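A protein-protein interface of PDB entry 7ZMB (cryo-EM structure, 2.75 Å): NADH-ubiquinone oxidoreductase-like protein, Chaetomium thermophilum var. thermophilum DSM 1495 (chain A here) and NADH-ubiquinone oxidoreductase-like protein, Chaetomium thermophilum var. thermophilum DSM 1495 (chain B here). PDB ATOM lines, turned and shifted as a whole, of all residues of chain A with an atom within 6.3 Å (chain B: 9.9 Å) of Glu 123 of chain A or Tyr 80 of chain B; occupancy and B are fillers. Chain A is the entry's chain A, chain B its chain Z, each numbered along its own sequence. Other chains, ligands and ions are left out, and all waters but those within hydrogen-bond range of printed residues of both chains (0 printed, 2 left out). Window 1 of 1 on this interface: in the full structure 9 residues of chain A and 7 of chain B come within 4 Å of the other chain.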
ATOM      1  N   MET A  86      22.843  33.734 -18.489  1.00  0.00           N
ATOM      2  CA  MET A  86      24.157  33.070 -18.604  1.00  0.00           C
ATOM      3  C   MET A  86      24.894  33.126 -17.270  1.00  0.00           C
ATOM      4  O   MET A  86      25.874  32.399 -17.100  1.00  0.00           O
ATOM      5  CB  MET A  86      24.989  33.730 -19.713  1.00  0.00           C
ATOM      6  CG  MET A  86      26.171  32.911 -20.189  1.00  0.00           C
ATOM      7  SD  MET A  86      25.737  31.220 -20.677  1.00  0.00           S
ATOM      8  CE  MET A  86      27.368  30.558 -20.995  1.00  0.00           C
ATOM      9  N   THR A 118      25.231  24.409 -12.586  1.00  0.00           N
ATOM     10  CA  THR A 118      25.734  25.518 -13.390  1.00  0.00           C
ATOM     11  C   THR A 118      26.207  25.035 -14.751  1.00  0.00           C
ATOM     12  O   THR A 118      26.023  25.729 -15.754  1.00  0.00           O
ATOM     13  CB  THR A 118      26.868  26.247 -12.666  1.00  0.00           C
ATOM     14  OG1 THR A 118      27.966  25.353 -12.460  1.00  0.00           O
ATOM     15  CG2 THR A 118      26.409  26.738 -11.325  1.00  0.00           C
ATOM     16  N   HIS A 119      26.824  23.851 -14.808  1.00  0.00           N
ATOM     17  CA  HIS A 119      27.204  23.283 -16.096  1.00  0.00           C
ATOM     18  C   HIS A 119      25.983  23.057 -16.971  1.00  0.00           C
ATOM     19  O   HIS A 119      26.005  23.352 -18.169  1.00  0.00           O
ATOM     20  CB  HIS A 119      27.953  21.966 -15.902  1.00  0.00           C
ATOM     21  CG  HIS A 119      29.317  22.119 -15.313  1.00  0.00           C
ATOM     22  ND1 HIS A 119      30.122  23.208 -15.567  1.00  0.00           N
ATOM     23  CD2 HIS A 119      30.021  21.320 -14.479  1.00  0.00           C
ATOM     24  CE1 HIS A 119      31.259  23.075 -14.913  1.00  0.00           C
ATOM     25  NE2 HIS A 119      31.223  21.939 -14.245  1.00  0.00           N
ATOM     26  N   LYS A 120      24.904  22.540 -16.387  1.00  0.00           N
ATOM     27  CA  LYS A 120      23.707  22.251 -17.167  1.00  0.00           C
ATOM     28  C   LYS A 120      23.026  23.526 -17.638  1.00  0.00           C
ATOM     29  O   LYS A 120      22.473  23.566 -18.740  1.00  0.00           O
ATOM     30  CB  LYS A 120      22.743  21.398 -16.352  1.00  0.00           C
ATOM     31  CG  LYS A 120      21.521  20.997 -17.129  1.00  0.00           C
ATOM     32  CD  LYS A 120      20.594  20.117 -16.341  1.00  0.00           C
ATOM     33  CE  LYS A 120      19.438  19.692 -17.219  1.00  0.00           C
ATOM     34  NZ  LYS A 120      18.587  20.881 -17.545  1.00  0.00           N
ATOM     35  N   ALA A 121      23.058  24.577 -16.820  1.00  0.00           N
ATOM     36  CA  ALA A 121      22.412  25.826 -17.201  1.00  0.00           C
ATOM     37  C   ALA A 121      23.188  26.544 -18.292  1.00  0.00           C
ATOM     38  O   ALA A 121      22.595  27.061 -19.244  1.00  0.00           O
ATOM     39  CB  ALA A 121      22.253  26.730 -15.984  1.00  0.00           C
ATOM     40  N   ARG A 122      24.510  26.610 -18.165  1.00  0.00           N
ATOM     41  CA  ARG A 122      25.299  27.342 -19.144  1.00  0.00           C
ATOM     42  C   ARG A 122      25.283  26.649 -20.499  1.00  0.00           C
ATOM     43  O   ARG A 122      25.223  27.314 -21.537  1.00  0.00           O
ATOM     44  CB  ARG A 122      26.724  27.514 -18.643  1.00  0.00           C
ATOM     45  CG  ARG A 122      26.824  28.303 -17.382  1.00  0.00           C
ATOM     46  CD  ARG A 122      28.198  28.198 -16.826  1.00  0.00           C
ATOM     47  NE  ARG A 122      28.346  28.972 -15.608  1.00  0.00           N
ATOM     48  CZ  ARG A 122      29.368  28.846 -14.777  1.00  0.00           C
ATOM     49  NH1 ARG A 122      30.317  27.970 -15.036  1.00  0.00           N
ATOM     50  NH2 ARG A 122      29.433  29.593 -13.691  1.00  0.00           N
ATOM     51  N   GLU A 123      25.266  25.318 -20.479  1.00  0.00           N
ATOM     52  CA  GLU A 123      25.181  24.545 -21.740  1.00  0.00           C
ATOM     53  C   GLU A 123      23.816  24.793 -22.387  1.00  0.00           C
ATOM     54  O   GLU A 123      23.812  25.114 -23.575  1.00  0.00           O
ATOM     55  CB  GLU A 123      25.600  23.086 -21.533  1.00  0.00           C
ATOM     56  CG  GLU A 123      27.020  22.793 -21.960  1.00  0.00           C
ATOM     57  CD  GLU A 123      27.646  21.562 -21.328  1.00  0.00           C
ATOM     58  OE1 GLU A 123      26.977  20.512 -21.288  1.00  0.00           O
ATOM     59  OE2 GLU A 123      28.795  21.663 -20.868  1.00  0.00           O
ATOM     60  N   GLY A 124      22.725  24.687 -21.636  1.00  0.00           N
ATOM     61  CA  GLY A 124      21.358  24.927 -22.143  1.00  0.00           C
ATOM     62  C   GLY A 124      21.046  26.335 -22.621  1.00  0.00           C
ATOM     63  O   GLY A 124      20.399  26.442 -23.636  1.00  0.00           O
ATOM     64  N   VAL A 125      21.473  27.366 -21.905  1.00  0.00           N
ATOM     65  CA  VAL A 125      21.323  28.790 -22.342  1.00  0.00           C
ATOM     66  C   VAL A 125      22.168  29.059 -23.587  1.00  0.00           C
ATOM     67  O   VAL A 125      21.702  29.770 -24.471  1.00  0.00           O
ATOM     68  CB  VAL A 125      21.532  29.821 -21.209  1.00  0.00           C
ATOM     69  CG1 VAL A 125      21.549  31.255 -21.707  1.00  0.00           C
ATOM     70  CG2 VAL A 125      20.498  29.666 -20.110  1.00  0.00           C
ATOM     71  N   MET A 126      23.353  28.484 -23.679  1.00  0.00           N
ATOM     72  CA  MET A 126      24.109  28.656 -24.938  1.00  0.00           C
ATOM     73  C   MET A 126      23.316  28.067 -26.111  1.00  0.00           C
ATOM     74  O   MET A 126      23.266  28.713 -27.138  1.00  0.00           O
ATOM     75  CB  MET A 126      25.515  28.059 -24.862  1.00  0.00           C
ATOM     76  CG  MET A 126      26.563  28.957 -24.209  1.00  0.00           C
ATOM     77  SD  MET A 126      26.557  30.714 -24.680  1.00  0.00           S
ATOM     78  CE  MET A 126      26.571  30.599 -26.466  1.00  0.00           C
ATOM     79  N   GLU A 127      22.653  26.920 -25.920  1.00  0.00           N
ATOM     80  CA  GLU A 127      21.851  26.297 -26.986  1.00  0.00           C
ATOM     81  C   GLU A 127      20.743  27.248 -27.421  1.00  0.00           C
ATOM     82  O   GLU A 127      20.568  27.406 -28.634  1.00  0.00           O
ATOM     83  CB  GLU A 127      21.243  24.984 -26.526  1.00  0.00           C
ATOM     84  CG  GLU A 127      20.567  24.221 -27.620  1.00  0.00           C
ATOM     85  CD  GLU A 127      20.190  22.849 -27.127  1.00  0.00           C
ATOM     86  OE1 GLU A 127      20.146  22.684 -25.899  1.00  0.00           O
ATOM     87  OE2 GLU A 127      19.968  21.959 -27.963  1.00  0.00           O
ATOM     88  N   PHE A 128      20.075  27.891 -26.473  1.00  0.00           N
ATOM     89  CA  PHE A 128      19.014  28.859 -26.806  1.00  0.00           C
ATOM     90  C   PHE A 128      19.564  30.079 -27.578  1.00  0.00           C
ATOM     91  O   PHE A 128      19.002  30.343 -28.620  1.00  0.00           O
ATOM     92  CB  PHE A 128      18.142  29.092 -25.567  1.00  0.00           C
ATOM     93  CG  PHE A 128      17.261  27.951 -25.144  1.00  0.00           C
ATOM     94  CD1 PHE A 128      16.402  27.347 -26.044  1.00  0.00           C
ATOM     95  CD2 PHE A 128      17.260  27.514 -23.832  1.00  0.00           C
ATOM     96  CE1 PHE A 128      15.582  26.309 -25.642  1.00  0.00           C
ATOM     97  CE2 PHE A 128      16.442  26.474 -23.432  1.00  0.00           C
ATOM     98  CZ  PHE A 128      15.606  25.876 -24.340  1.00  0.00           C
ATOM     99  N   MET A 153      32.490  28.486 -26.725  1.00  0.00           N
ATOM    100  CA  MET A 153      33.562  27.499 -26.699  1.00  0.00           C
ATOM    101  C   MET A 153      33.877  27.043 -25.279  1.00  0.00           C
ATOM    102  O   MET A 153      34.222  25.876 -25.068  1.00  0.00           O
ATOM    103  CB  MET A 153      34.808  28.075 -27.382  1.00  0.00           C
ATOM    104  CG  MET A 153      36.096  27.299 -27.173  1.00  0.00           C
ATOM    105  SD  MET A 153      36.247  25.774 -28.118  1.00  0.00           S
ATOM    106  CE  MET A 153      35.967  26.336 -29.796  1.00  0.00           C
ATOM    107  N   ARG A 154      33.739  27.928 -24.295  1.00  0.00           N
ATOM    108  CA  ARG A 154      34.068  27.612 -22.911  1.00  0.00           C
ATOM    109  C   ARG A 154      32.902  27.017 -22.129  1.00  0.00           C
ATOM    110  O   ARG A 154      33.128  26.254 -21.187  1.00  0.00           O
ATOM    111  CB  ARG A 154      34.571  28.873 -22.204  1.00  0.00           C
ATOM    112  CG  ARG A 154      34.893  28.720 -20.738  1.00  0.00           C
ATOM    113  CD  ARG A 154      36.007  27.727 -20.536  1.00  0.00           C
ATOM    114  NE  ARG A 154      36.448  27.654 -19.153  1.00  0.00           N
ATOM    115  CZ  ARG A 154      36.025  26.749 -18.283  1.00  0.00           C
ATOM    116  NH1 ARG A 154      36.487  26.759 -17.046  1.00  0.00           N
ATOM    117  NH2 ARG A 154      35.135  25.843 -18.646  1.00  0.00           N
ATOM    118  N   TYR A 155      31.663  27.332 -22.486  1.00  0.00           N
ATOM    119  CA  TYR A 155      30.536  26.976 -21.640  1.00  0.00           C
ATOM    120  C   TYR A 155      29.418  26.225 -22.335  1.00  0.00           C
ATOM    121  O   TYR A 155      28.539  25.713 -21.642  1.00  0.00           O
ATOM    122  CB  TYR A 155      29.952  28.230 -20.980  1.00  0.00           C
ATOM    123  CG  TYR A 155      30.910  28.874 -20.025  1.00  0.00           C
ATOM    124  CD1 TYR A 155      31.252  28.242 -18.842  1.00  0.00           C
ATOM    125  CD2 TYR A 155      31.502  30.091 -20.314  1.00  0.00           C
ATOM    126  CE1 TYR A 155      32.139  28.806 -17.966  1.00  0.00           C
ATOM    127  CE2 TYR A 155      32.385  30.670 -19.436  1.00  0.00           C
ATOM    128  CZ  TYR A 155      32.701  30.017 -18.263  1.00  0.00           C
ATOM    129  OH  TYR A 155      33.586  30.573 -17.380  1.00  0.00           O
ATOM    130  N   GLY A 156      29.416  26.128 -23.663  1.00  0.00           N
ATOM    131  CA  GLY A 156      28.398  25.392 -24.372  1.00  0.00           C
ATOM    132  C   GLY A 156      28.901  24.045 -24.860  1.00  0.00           C
ATOM    133  O   GLY A 156      30.072  23.704 -24.752  1.00  0.00           O
ATOM    134  N   ALA A 157      27.973  23.274 -25.411  1.00  0.00           N
ATOM    135  CA  ALA A 157      28.342  22.052 -26.100  1.00  0.00           C
ATOM    136  C   ALA A 157      29.138  22.389 -27.351  1.00  0.00           C
ATOM    137  O   ALA A 157      29.146  23.525 -27.824  1.00  0.00           O
ATOM    138  CB  ALA A 157      27.100  21.244 -26.467  1.00  0.00           C
ATOM    139  N   ASP A 158      29.848  21.412 -27.871  1.00  0.00           N
ATOM    140  CA  ASP A 158      30.617  21.621 -29.116  1.00  0.00           C
ATOM    141  C   ASP A 158      29.714  21.574 -30.348  1.00  0.00           C
ATOM    142  O   ASP A 158      30.177  22.018 -31.403  1.00  0.00           O
ATOM    143  CB  ASP A 158      31.733  20.584 -29.237  1.00  0.00           C
ATOM    144  CG  ASP A 158      31.256  19.149 -29.329  1.00  0.00           C
ATOM    145  OD1 ASP A 158      30.434  18.757 -28.497  1.00  0.00           O
ATOM    146  OD2 ASP A 158      31.704  18.445 -30.241  1.00  0.00           O
ATOM    147  N   PRO B  71      26.993   7.971 -27.938  1.00  0.00           N
ATOM    148  CA  PRO B  71      26.908   8.956 -26.850  1.00  0.00           C
ATOM    149  C   PRO B  71      27.336  10.341 -27.303  1.00  0.00           C
ATOM    150  O   PRO B  71      26.534  11.272 -27.236  1.00  0.00           O
ATOM    151  CB  PRO B  71      27.845   8.392 -25.771  1.00  0.00           C
ATOM    152  CG  PRO B  71      28.202   7.042 -26.221  1.00  0.00           C
ATOM    153  CD  PRO B  71      28.080   7.012 -27.697  1.00  0.00           C
ATOM    154  N   ALA B  72      28.578  10.495 -27.786  1.00  0.00           N
ATOM    155  CA  ALA B  72      29.144  11.793 -28.229  1.00  0.00           C
ATOM    156  C   ALA B  72      28.258  12.459 -29.283  1.00  0.00           C
ATOM    157  O   ALA B  72      28.048  13.689 -29.208  1.00  0.00           O
ATOM    158  CB  ALA B  72      30.567  11.682 -28.648  1.00  0.00           C
ATOM    159  N   GLY B  73      27.768  11.690 -30.243  1.00  0.00           N
ATOM    160  CA  GLY B  73      26.979  12.243 -31.325  1.00  0.00           C
ATOM    161  C   GLY B  73      25.481  12.249 -31.140  1.00  0.00           C
ATOM    162  O   GLY B  73      24.777  12.782 -31.996  1.00  0.00           O
ATOM    163  N   ASP B  74      24.974  11.692 -30.042  1.00  0.00           N
ATOM    164  CA  ASP B  74      23.538  11.629 -29.806  1.00  0.00           C
ATOM    165  C   ASP B  74      22.957  13.026 -29.608  1.00  0.00           C
ATOM    166  O   ASP B  74      23.655  13.971 -29.241  1.00  0.00           O
ATOM    167  CB  ASP B  74      23.239  10.776 -28.573  1.00  0.00           C
ATOM    168  CG  ASP B  74      21.816  10.295 -28.528  1.00  0.00           C
ATOM    169  OD1 ASP B  74      21.501   9.299 -29.206  1.00  0.00           O
ATOM    170  OD2 ASP B  74      21.007  10.905 -27.801  1.00  0.00           O
ATOM    171  N   ALA B  76      20.249  13.365 -27.482  1.00  0.00           N
ATOM    172  CA  ALA B  76      19.517  13.433 -26.222  1.00  0.00           C
ATOM    173  C   ALA B  76      20.121  12.658 -25.052  1.00  0.00           C
ATOM    174  O   ALA B  76      19.383  12.347 -24.111  1.00  0.00           O
ATOM    175  CB  ALA B  76      18.083  12.947 -26.423  1.00  0.00           C
ATOM    176  N   ASP B  77      21.395  12.293 -25.062  1.00  0.00           N
ATOM    177  CA  ASP B  77      21.912  11.609 -23.880  1.00  0.00           C
ATOM    178  C   ASP B  77      23.335  12.036 -23.555  1.00  0.00           C
ATOM    179  O   ASP B  77      24.124  11.248 -23.025  1.00  0.00           O
ATOM    180  CB  ASP B  77      21.848  10.092 -24.041  1.00  0.00           C
ATOM    181  CG  ASP B  77      21.783   9.369 -22.710  1.00  0.00           C
ATOM    182  OD1 ASP B  77      21.711  10.050 -21.666  1.00  0.00           O
ATOM    183  OD2 ASP B  77      21.805   8.120 -22.707  1.00  0.00           O
ATOM    184  N   ASN B  78      23.700  13.262 -23.856  1.00  0.00           N
ATOM    185  CA  ASN B  78      25.052  13.727 -23.556  1.00  0.00           C
ATOM    186  C   ASN B  78      25.069  15.230 -23.367  1.00  0.00           C
ATOM    187  O   ASN B  78      25.039  15.997 -24.340  1.00  0.00           O
ATOM    188  CB  ASN B  78      26.052  13.307 -24.630  1.00  0.00           C
ATOM    189  CG  ASN B  78      25.627  13.711 -26.006  1.00  0.00           C
ATOM    190  OD1 ASN B  78      24.452  13.620 -26.355  1.00  0.00           O
ATOM    191  ND2 ASN B  78      26.579  14.155 -26.808  1.00  0.00           N
ATOM    192  N   PRO B  79      25.102  15.695 -22.127  1.00  0.00           N
ATOM    193  CA  PRO B  79      25.691  17.006 -21.868  1.00  0.00           C
ATOM    194  C   PRO B  79      27.171  16.960 -22.198  1.00  0.00           C
ATOM    195  O   PRO B  79      27.825  15.922 -22.079  1.00  0.00           O
ATOM    196  CB  PRO B  79      25.452  17.218 -20.373  1.00  0.00           C
ATOM    197  CG  PRO B  79      25.246  15.884 -19.837  1.00  0.00           C
ATOM    198  CD  PRO B  79      24.566  15.089 -20.903  1.00  0.00           C
ATOM    199  N   TYR B  80      27.701  18.096 -22.636  1.00  0.00           N
ATOM    200  CA  TYR B  80      29.115  18.127 -22.966  1.00  0.00           C
ATOM    201  C   TYR B  80      29.977  17.938 -21.727  1.00  0.00           C
ATOM    202  O   TYR B  80      31.045  17.323 -21.809  1.00  0.00           O
ATOM    203  CB  TYR B  80      29.467  19.427 -23.686  1.00  0.00           C
ATOM    204  CG  TYR B  80      30.934  19.552 -23.960  1.00  0.00           C
ATOM    205  CD1 TYR B  80      31.517  18.889 -25.026  1.00  0.00           C
ATOM    206  CD2 TYR B  80      31.748  20.296 -23.127  1.00  0.00           C
ATOM    207  CE1 TYR B  80      32.859  18.985 -25.264  1.00  0.00           C
ATOM    208  CE2 TYR B  80      33.092  20.398 -23.361  1.00  0.00           C
ATOM    209  CZ  TYR B  80      33.644  19.740 -24.426  1.00  0.00           C
ATOM    210  OH  TYR B  80      34.993  19.847 -24.650  1.00  0.00           O
ATOM    211  N   TRP B  81      29.527  18.423 -20.573  1.00  0.00           N
ATOM    212  CA  TRP B  81      30.390  18.461 -19.402  1.00  0.00           C
ATOM    213  C   TRP B  81      30.687  17.086 -18.815  1.00  0.00           C
ATOM    214  O   TRP B  81      31.642  16.967 -18.041  1.00  0.00           O
ATOM    215  CB  TRP B  81      29.791  19.363 -18.325  1.00  0.00           C
ATOM    216  CG  TRP B  81      28.462  18.930 -17.828  1.00  0.00           C
ATOM    217  CD1 TRP B  81      27.254  19.250 -18.351  1.00  0.00           C
ATOM    218  CD2 TRP B  81      28.203  18.101 -16.697  1.00  0.00           C
ATOM    219  NE1 TRP B  81      26.256  18.676 -17.621  1.00  0.00           N
ATOM    220  CE2 TRP B  81      26.810  17.962 -16.595  1.00  0.00           C
ATOM    221  CE3 TRP B  81      29.016  17.470 -15.751  1.00  0.00           C
ATOM    222  CZ2 TRP B  81      26.205  17.208 -15.596  1.00  0.00           C
ATOM    223  CZ3 TRP B  81      28.416  16.723 -14.761  1.00  0.00           C
ATOM    224  CH2 TRP B  81      27.021  16.598 -14.689  1.00  0.00           C
ATOM    225  N   LYS B  82      29.921  16.050 -19.151  1.00  0.00           N
ATOM    226  CA  LYS B  82      30.273  14.711 -18.702  1.00  0.00           C
ATOM    227  C   LYS B  82      31.219  13.999 -19.657  1.00  0.00           C
ATOM    228  O   LYS B  82      31.600  12.859 -19.394  1.00  0.00           O
ATOM    229  CB  LYS B  82      29.032  13.849 -18.469  1.00  0.00           C
ATOM    230  CG  LYS B  82      28.162  14.295 -17.313  1.00  0.00           C
ATOM    231  CD  LYS B  82      27.102  13.257 -16.978  1.00  0.00           C
ATOM    232  CE  LYS B  82      25.992  13.178 -17.993  1.00  0.00           C
ATOM    233  NZ  LYS B  82      24.920  12.233 -17.583  1.00  0.00           N
ATOM    234  N   ARG B  83      31.695  14.684 -20.683  1.00  0.00           N
ATOM    235  CA  ARG B  83      32.682  14.121 -21.634  1.00  0.00           C
ATOM    236  C   ARG B  83      33.803  15.158 -21.818  1.00  0.00           C
ATOM    237  O   ARG B  83      34.650  14.969 -22.707  1.00  0.00           O
ATOM    238  CB  ARG B  83      31.987  13.718 -22.944  1.00  0.00           C
ATOM    239  CG  ARG B  83      31.231  14.795 -23.699  1.00  0.00           C
ATOM    240  CD  ARG B  83      30.533  14.157 -24.888  1.00  0.00           C
ATOM    241  NE  ARG B  83      29.716  15.095 -25.645  1.00  0.00           N
ATOM    242  CZ  ARG B  83      30.042  15.611 -26.820  1.00  0.00           C
ATOM    243  NH1 ARG B  83      29.229  16.469 -27.410  1.00  0.00           N
ATOM    244  NH2 ARG B  83      31.171  15.270 -27.409  1.00  0.00           N
ATOM    245  N   ASP B  84      33.794  16.223 -21.021  1.00  0.00           N
ATOM    246  CA  ASP B  84      34.778  17.289 -21.171  1.00  0.00           C
ATOM    247  C   ASP B  84      36.044  16.856 -20.429  1.00  0.00           C
ATOM    248  O   ASP B  84      36.423  17.385 -19.381  1.00  0.00           O
ATOM    249  CB  ASP B  84      34.209  18.597 -20.640  1.00  0.00           C
ATOM    250  CG  ASP B  84      35.148  19.770 -20.797  1.00  0.00           C
ATOM    251  OD1 ASP B  84      36.363  19.593 -20.998  1.00  0.00           O
ATOM    252  OD2 ASP B  84      34.647  20.904 -20.718  1.00  0.00           O
ATOM    253  N   PHE B  85      36.693  15.843 -20.994  1.00  0.00           N
ATOM    254  CA  PHE B  85      37.850  15.248 -20.350  1.00  0.00           C
ATOM    255  C   PHE B  85      39.078  16.141 -20.434  1.00  0.00           C
ATOM    256  O   PHE B  85      40.023  15.941 -19.666  1.00  0.00           O
ATOM    257  CB  PHE B  85      38.138  13.889 -20.977  1.00  0.00           C
ATOM    258  CG  PHE B  85      37.062  12.880 -20.748  1.00  0.00           C
ATOM    259  CD1 PHE B  85      36.693  12.520 -19.472  1.00  0.00           C
ATOM    260  CD2 PHE B  85      36.428  12.279 -21.813  1.00  0.00           C
ATOM    261  CE1 PHE B  85      35.707  11.591 -19.268  1.00  0.00           C
ATOM    262  CE2 PHE B  85      35.445  11.353 -21.608  1.00  0.00           C
ATOM    263  CZ  PHE B  85      35.088  11.010 -20.333  1.00  0.00           C
ATOM    264  N   ARG B  86      39.089  17.108 -21.354  1.00  0.00           N
ATOM    265  CA  ARG B  86      40.213  18.030 -21.438  1.00  0.00           C
ATOM    266  C   ARG B  86      40.255  18.960 -20.236  1.00  0.00           C
ATOM    267  O   ARG B  86      41.332  19.275 -19.722  1.00  0.00           O
ATOM    268  CB  ARG B  86      40.146  18.826 -22.735  1.00  0.00           C
ATOM    269  CG  ARG B  86      41.139  19.972 -22.823  1.00  0.00           C
ATOM    270  CD  ARG B  86      41.047  20.692 -24.132  1.00  0.00           C
ATOM    271  NE  ARG B  86      39.720  21.245 -24.382  1.00  0.00           N
ATOM    272  CZ  ARG B  86      39.489  22.478 -24.824  1.00  0.00           C
ATOM    273  NH1 ARG B  86      38.248  22.879 -25.031  1.00  0.00           N
ATOM    274  NH2 ARG B  86      40.493  23.305 -25.071  1.00  0.00           N
ATOM    275  N   ARG B  87      39.099  19.411 -19.771  1.00  0.00           N
ATOM    276  CA  ARG B  87      39.040  20.291 -18.619  1.00  0.00           C
ATOM    277  C   ARG B  87      39.032  19.530 -17.304  1.00  0.00           C
ATOM    278  O   ARG B  87      39.126  20.146 -16.241  1.00  0.00           O
ATOM    279  CB  ARG B  87      37.816  21.196 -18.720  1.00  0.00           C
ATOM    280  CG  ARG B  87      38.000  22.294 -19.746  1.00  0.00           C
ATOM    281  CD  ARG B  87      36.728  23.052 -19.988  1.00  0.00           C
ATOM    282  NE  ARG B  87      36.834  23.895 -21.170  1.00  0.00           N
ATOM    283  CZ  ARG B  87      35.922  23.955 -22.131  1.00  0.00           C
ATOM    284  NH1 ARG B  87      34.823  23.224 -22.058  1.00  0.00           N
ATOM    285  NH2 ARG B  87      36.112  24.757 -23.161  1.00  0.00           N
ATOM    286  N   ASN B  88      38.941  18.207 -17.357  1.00  0.00           N
ATOM    287  CA  ASN B  88      39.167  17.362 -16.196  1.00  0.00           C
ATOM    288  C   ASN B  88      40.606  16.884 -16.113  1.00  0.00           C
ATOM    289  O   ASN B  88      40.867  15.799 -15.584  1.00  0.00           O
ATOM    290  CB  ASN B  88      38.195  16.184 -16.223  1.00  0.00           C
ATOM    291  CG  ASN B  88      36.810  16.577 -15.767  1.00  0.00           C
ATOM    292  OD1 ASN B  88      36.319  16.088 -14.756  1.00  0.00           O
ATOM    293  ND2 ASN B  88      36.174  17.472 -16.504  1.00  0.00           N
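Printed residues of chain B that touch a printed residue of chain A: Pro 79, Tyr 80, Trp 81, Arg 83 and Arg 87. Hydrophobic or aromatic side chains of chain B within 4 Å of the printed part of chain A: Pro 79, Tyr 80 and Trp 81. Hydrophobic or aromatic side chains of chain A within 4 Å of the printed part of chain B: His 119. Among the printed residues, 9 pairs touch across the chains.
Among the printed residues, pairs that only touch across the chains: His 119 of chain A with Trp 81 of chain B, Glu 123 of chain A with Pro 79 of chain B, Arg 154 of chain A with Arg 87 of chain B, Ala 157 of chain A with Tyr 80 of chain B and Asp 158 of chain A with Tyr 80 of chain B.
N of Tyr 80 of chain B is in hydrogen-bond range of OE1 of Glu 123 of chain A. N of Trp 81 of chain B lies within hydrogen-bond range of OE2 of Glu 123 of chain A (3.3 Å). OD1 of Asp 158 of chain A lies within salt-bridge range of NH1 of Arg 83 of chain B, 2.8 Å away. The backbone carbonyl oxygen (O) of Met 153 of chain A sits at hydrogen-bond distance from the guanidinium group (NH2) of Arg 87 of chain B (2.9 Å).
Of the printed residues of chain B, His 119 of chain A touches Trp 81. Ala 121 of chain A touches none of the printed residues of chain B. Arg 122 of chain A touches none of the printed residues of chain B. No residue of chain B comes within 4 Å of Gly 124 of chain A. No residue of chain B comes within 4 Å of Gly 156 of chain A. Of chain B, only Tyr 80 (3.7 Å) comes within 4 Å of Ala 157 of chain A. Ala 72 of chain B touches none of the printed residues of chain A. Tyr 80 of chain B touches just these residues of chain A: Glu 123 (2.9 Å), Ala 157 (3.7 Å) and Asp 158 (3.6 Å). Printed residues of chain A within 4 Å of Trp 81 of chain B: His 119 (3.6 Å) and Glu 123 (3.2 Å). Printed residues of chain A within 4 Å of Arg 87 of chain B: Met 153 and Arg 154. The nearest residue of chain A that does not touch Tyr 80 of chain B is Gly 156 of chain A (4.1 Å).
The guanidinium group (NE) of Arg 83 of chain B lies close to the side-chain amide nitrogen (ND2) of Asn 78 of chain B (3.5 Å). The side-chain carboxylate (OD2) of Asp 84 of chain B is in salt-bridge range of the guanidinium group (NH1) of Arg 87 of chain B (2.7 Å). The backbone NH (N) of Glu 123 of chain A lies close to the backbone carbonyl oxygen (O) of Tyr 155 of chain A (3.5 Å).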
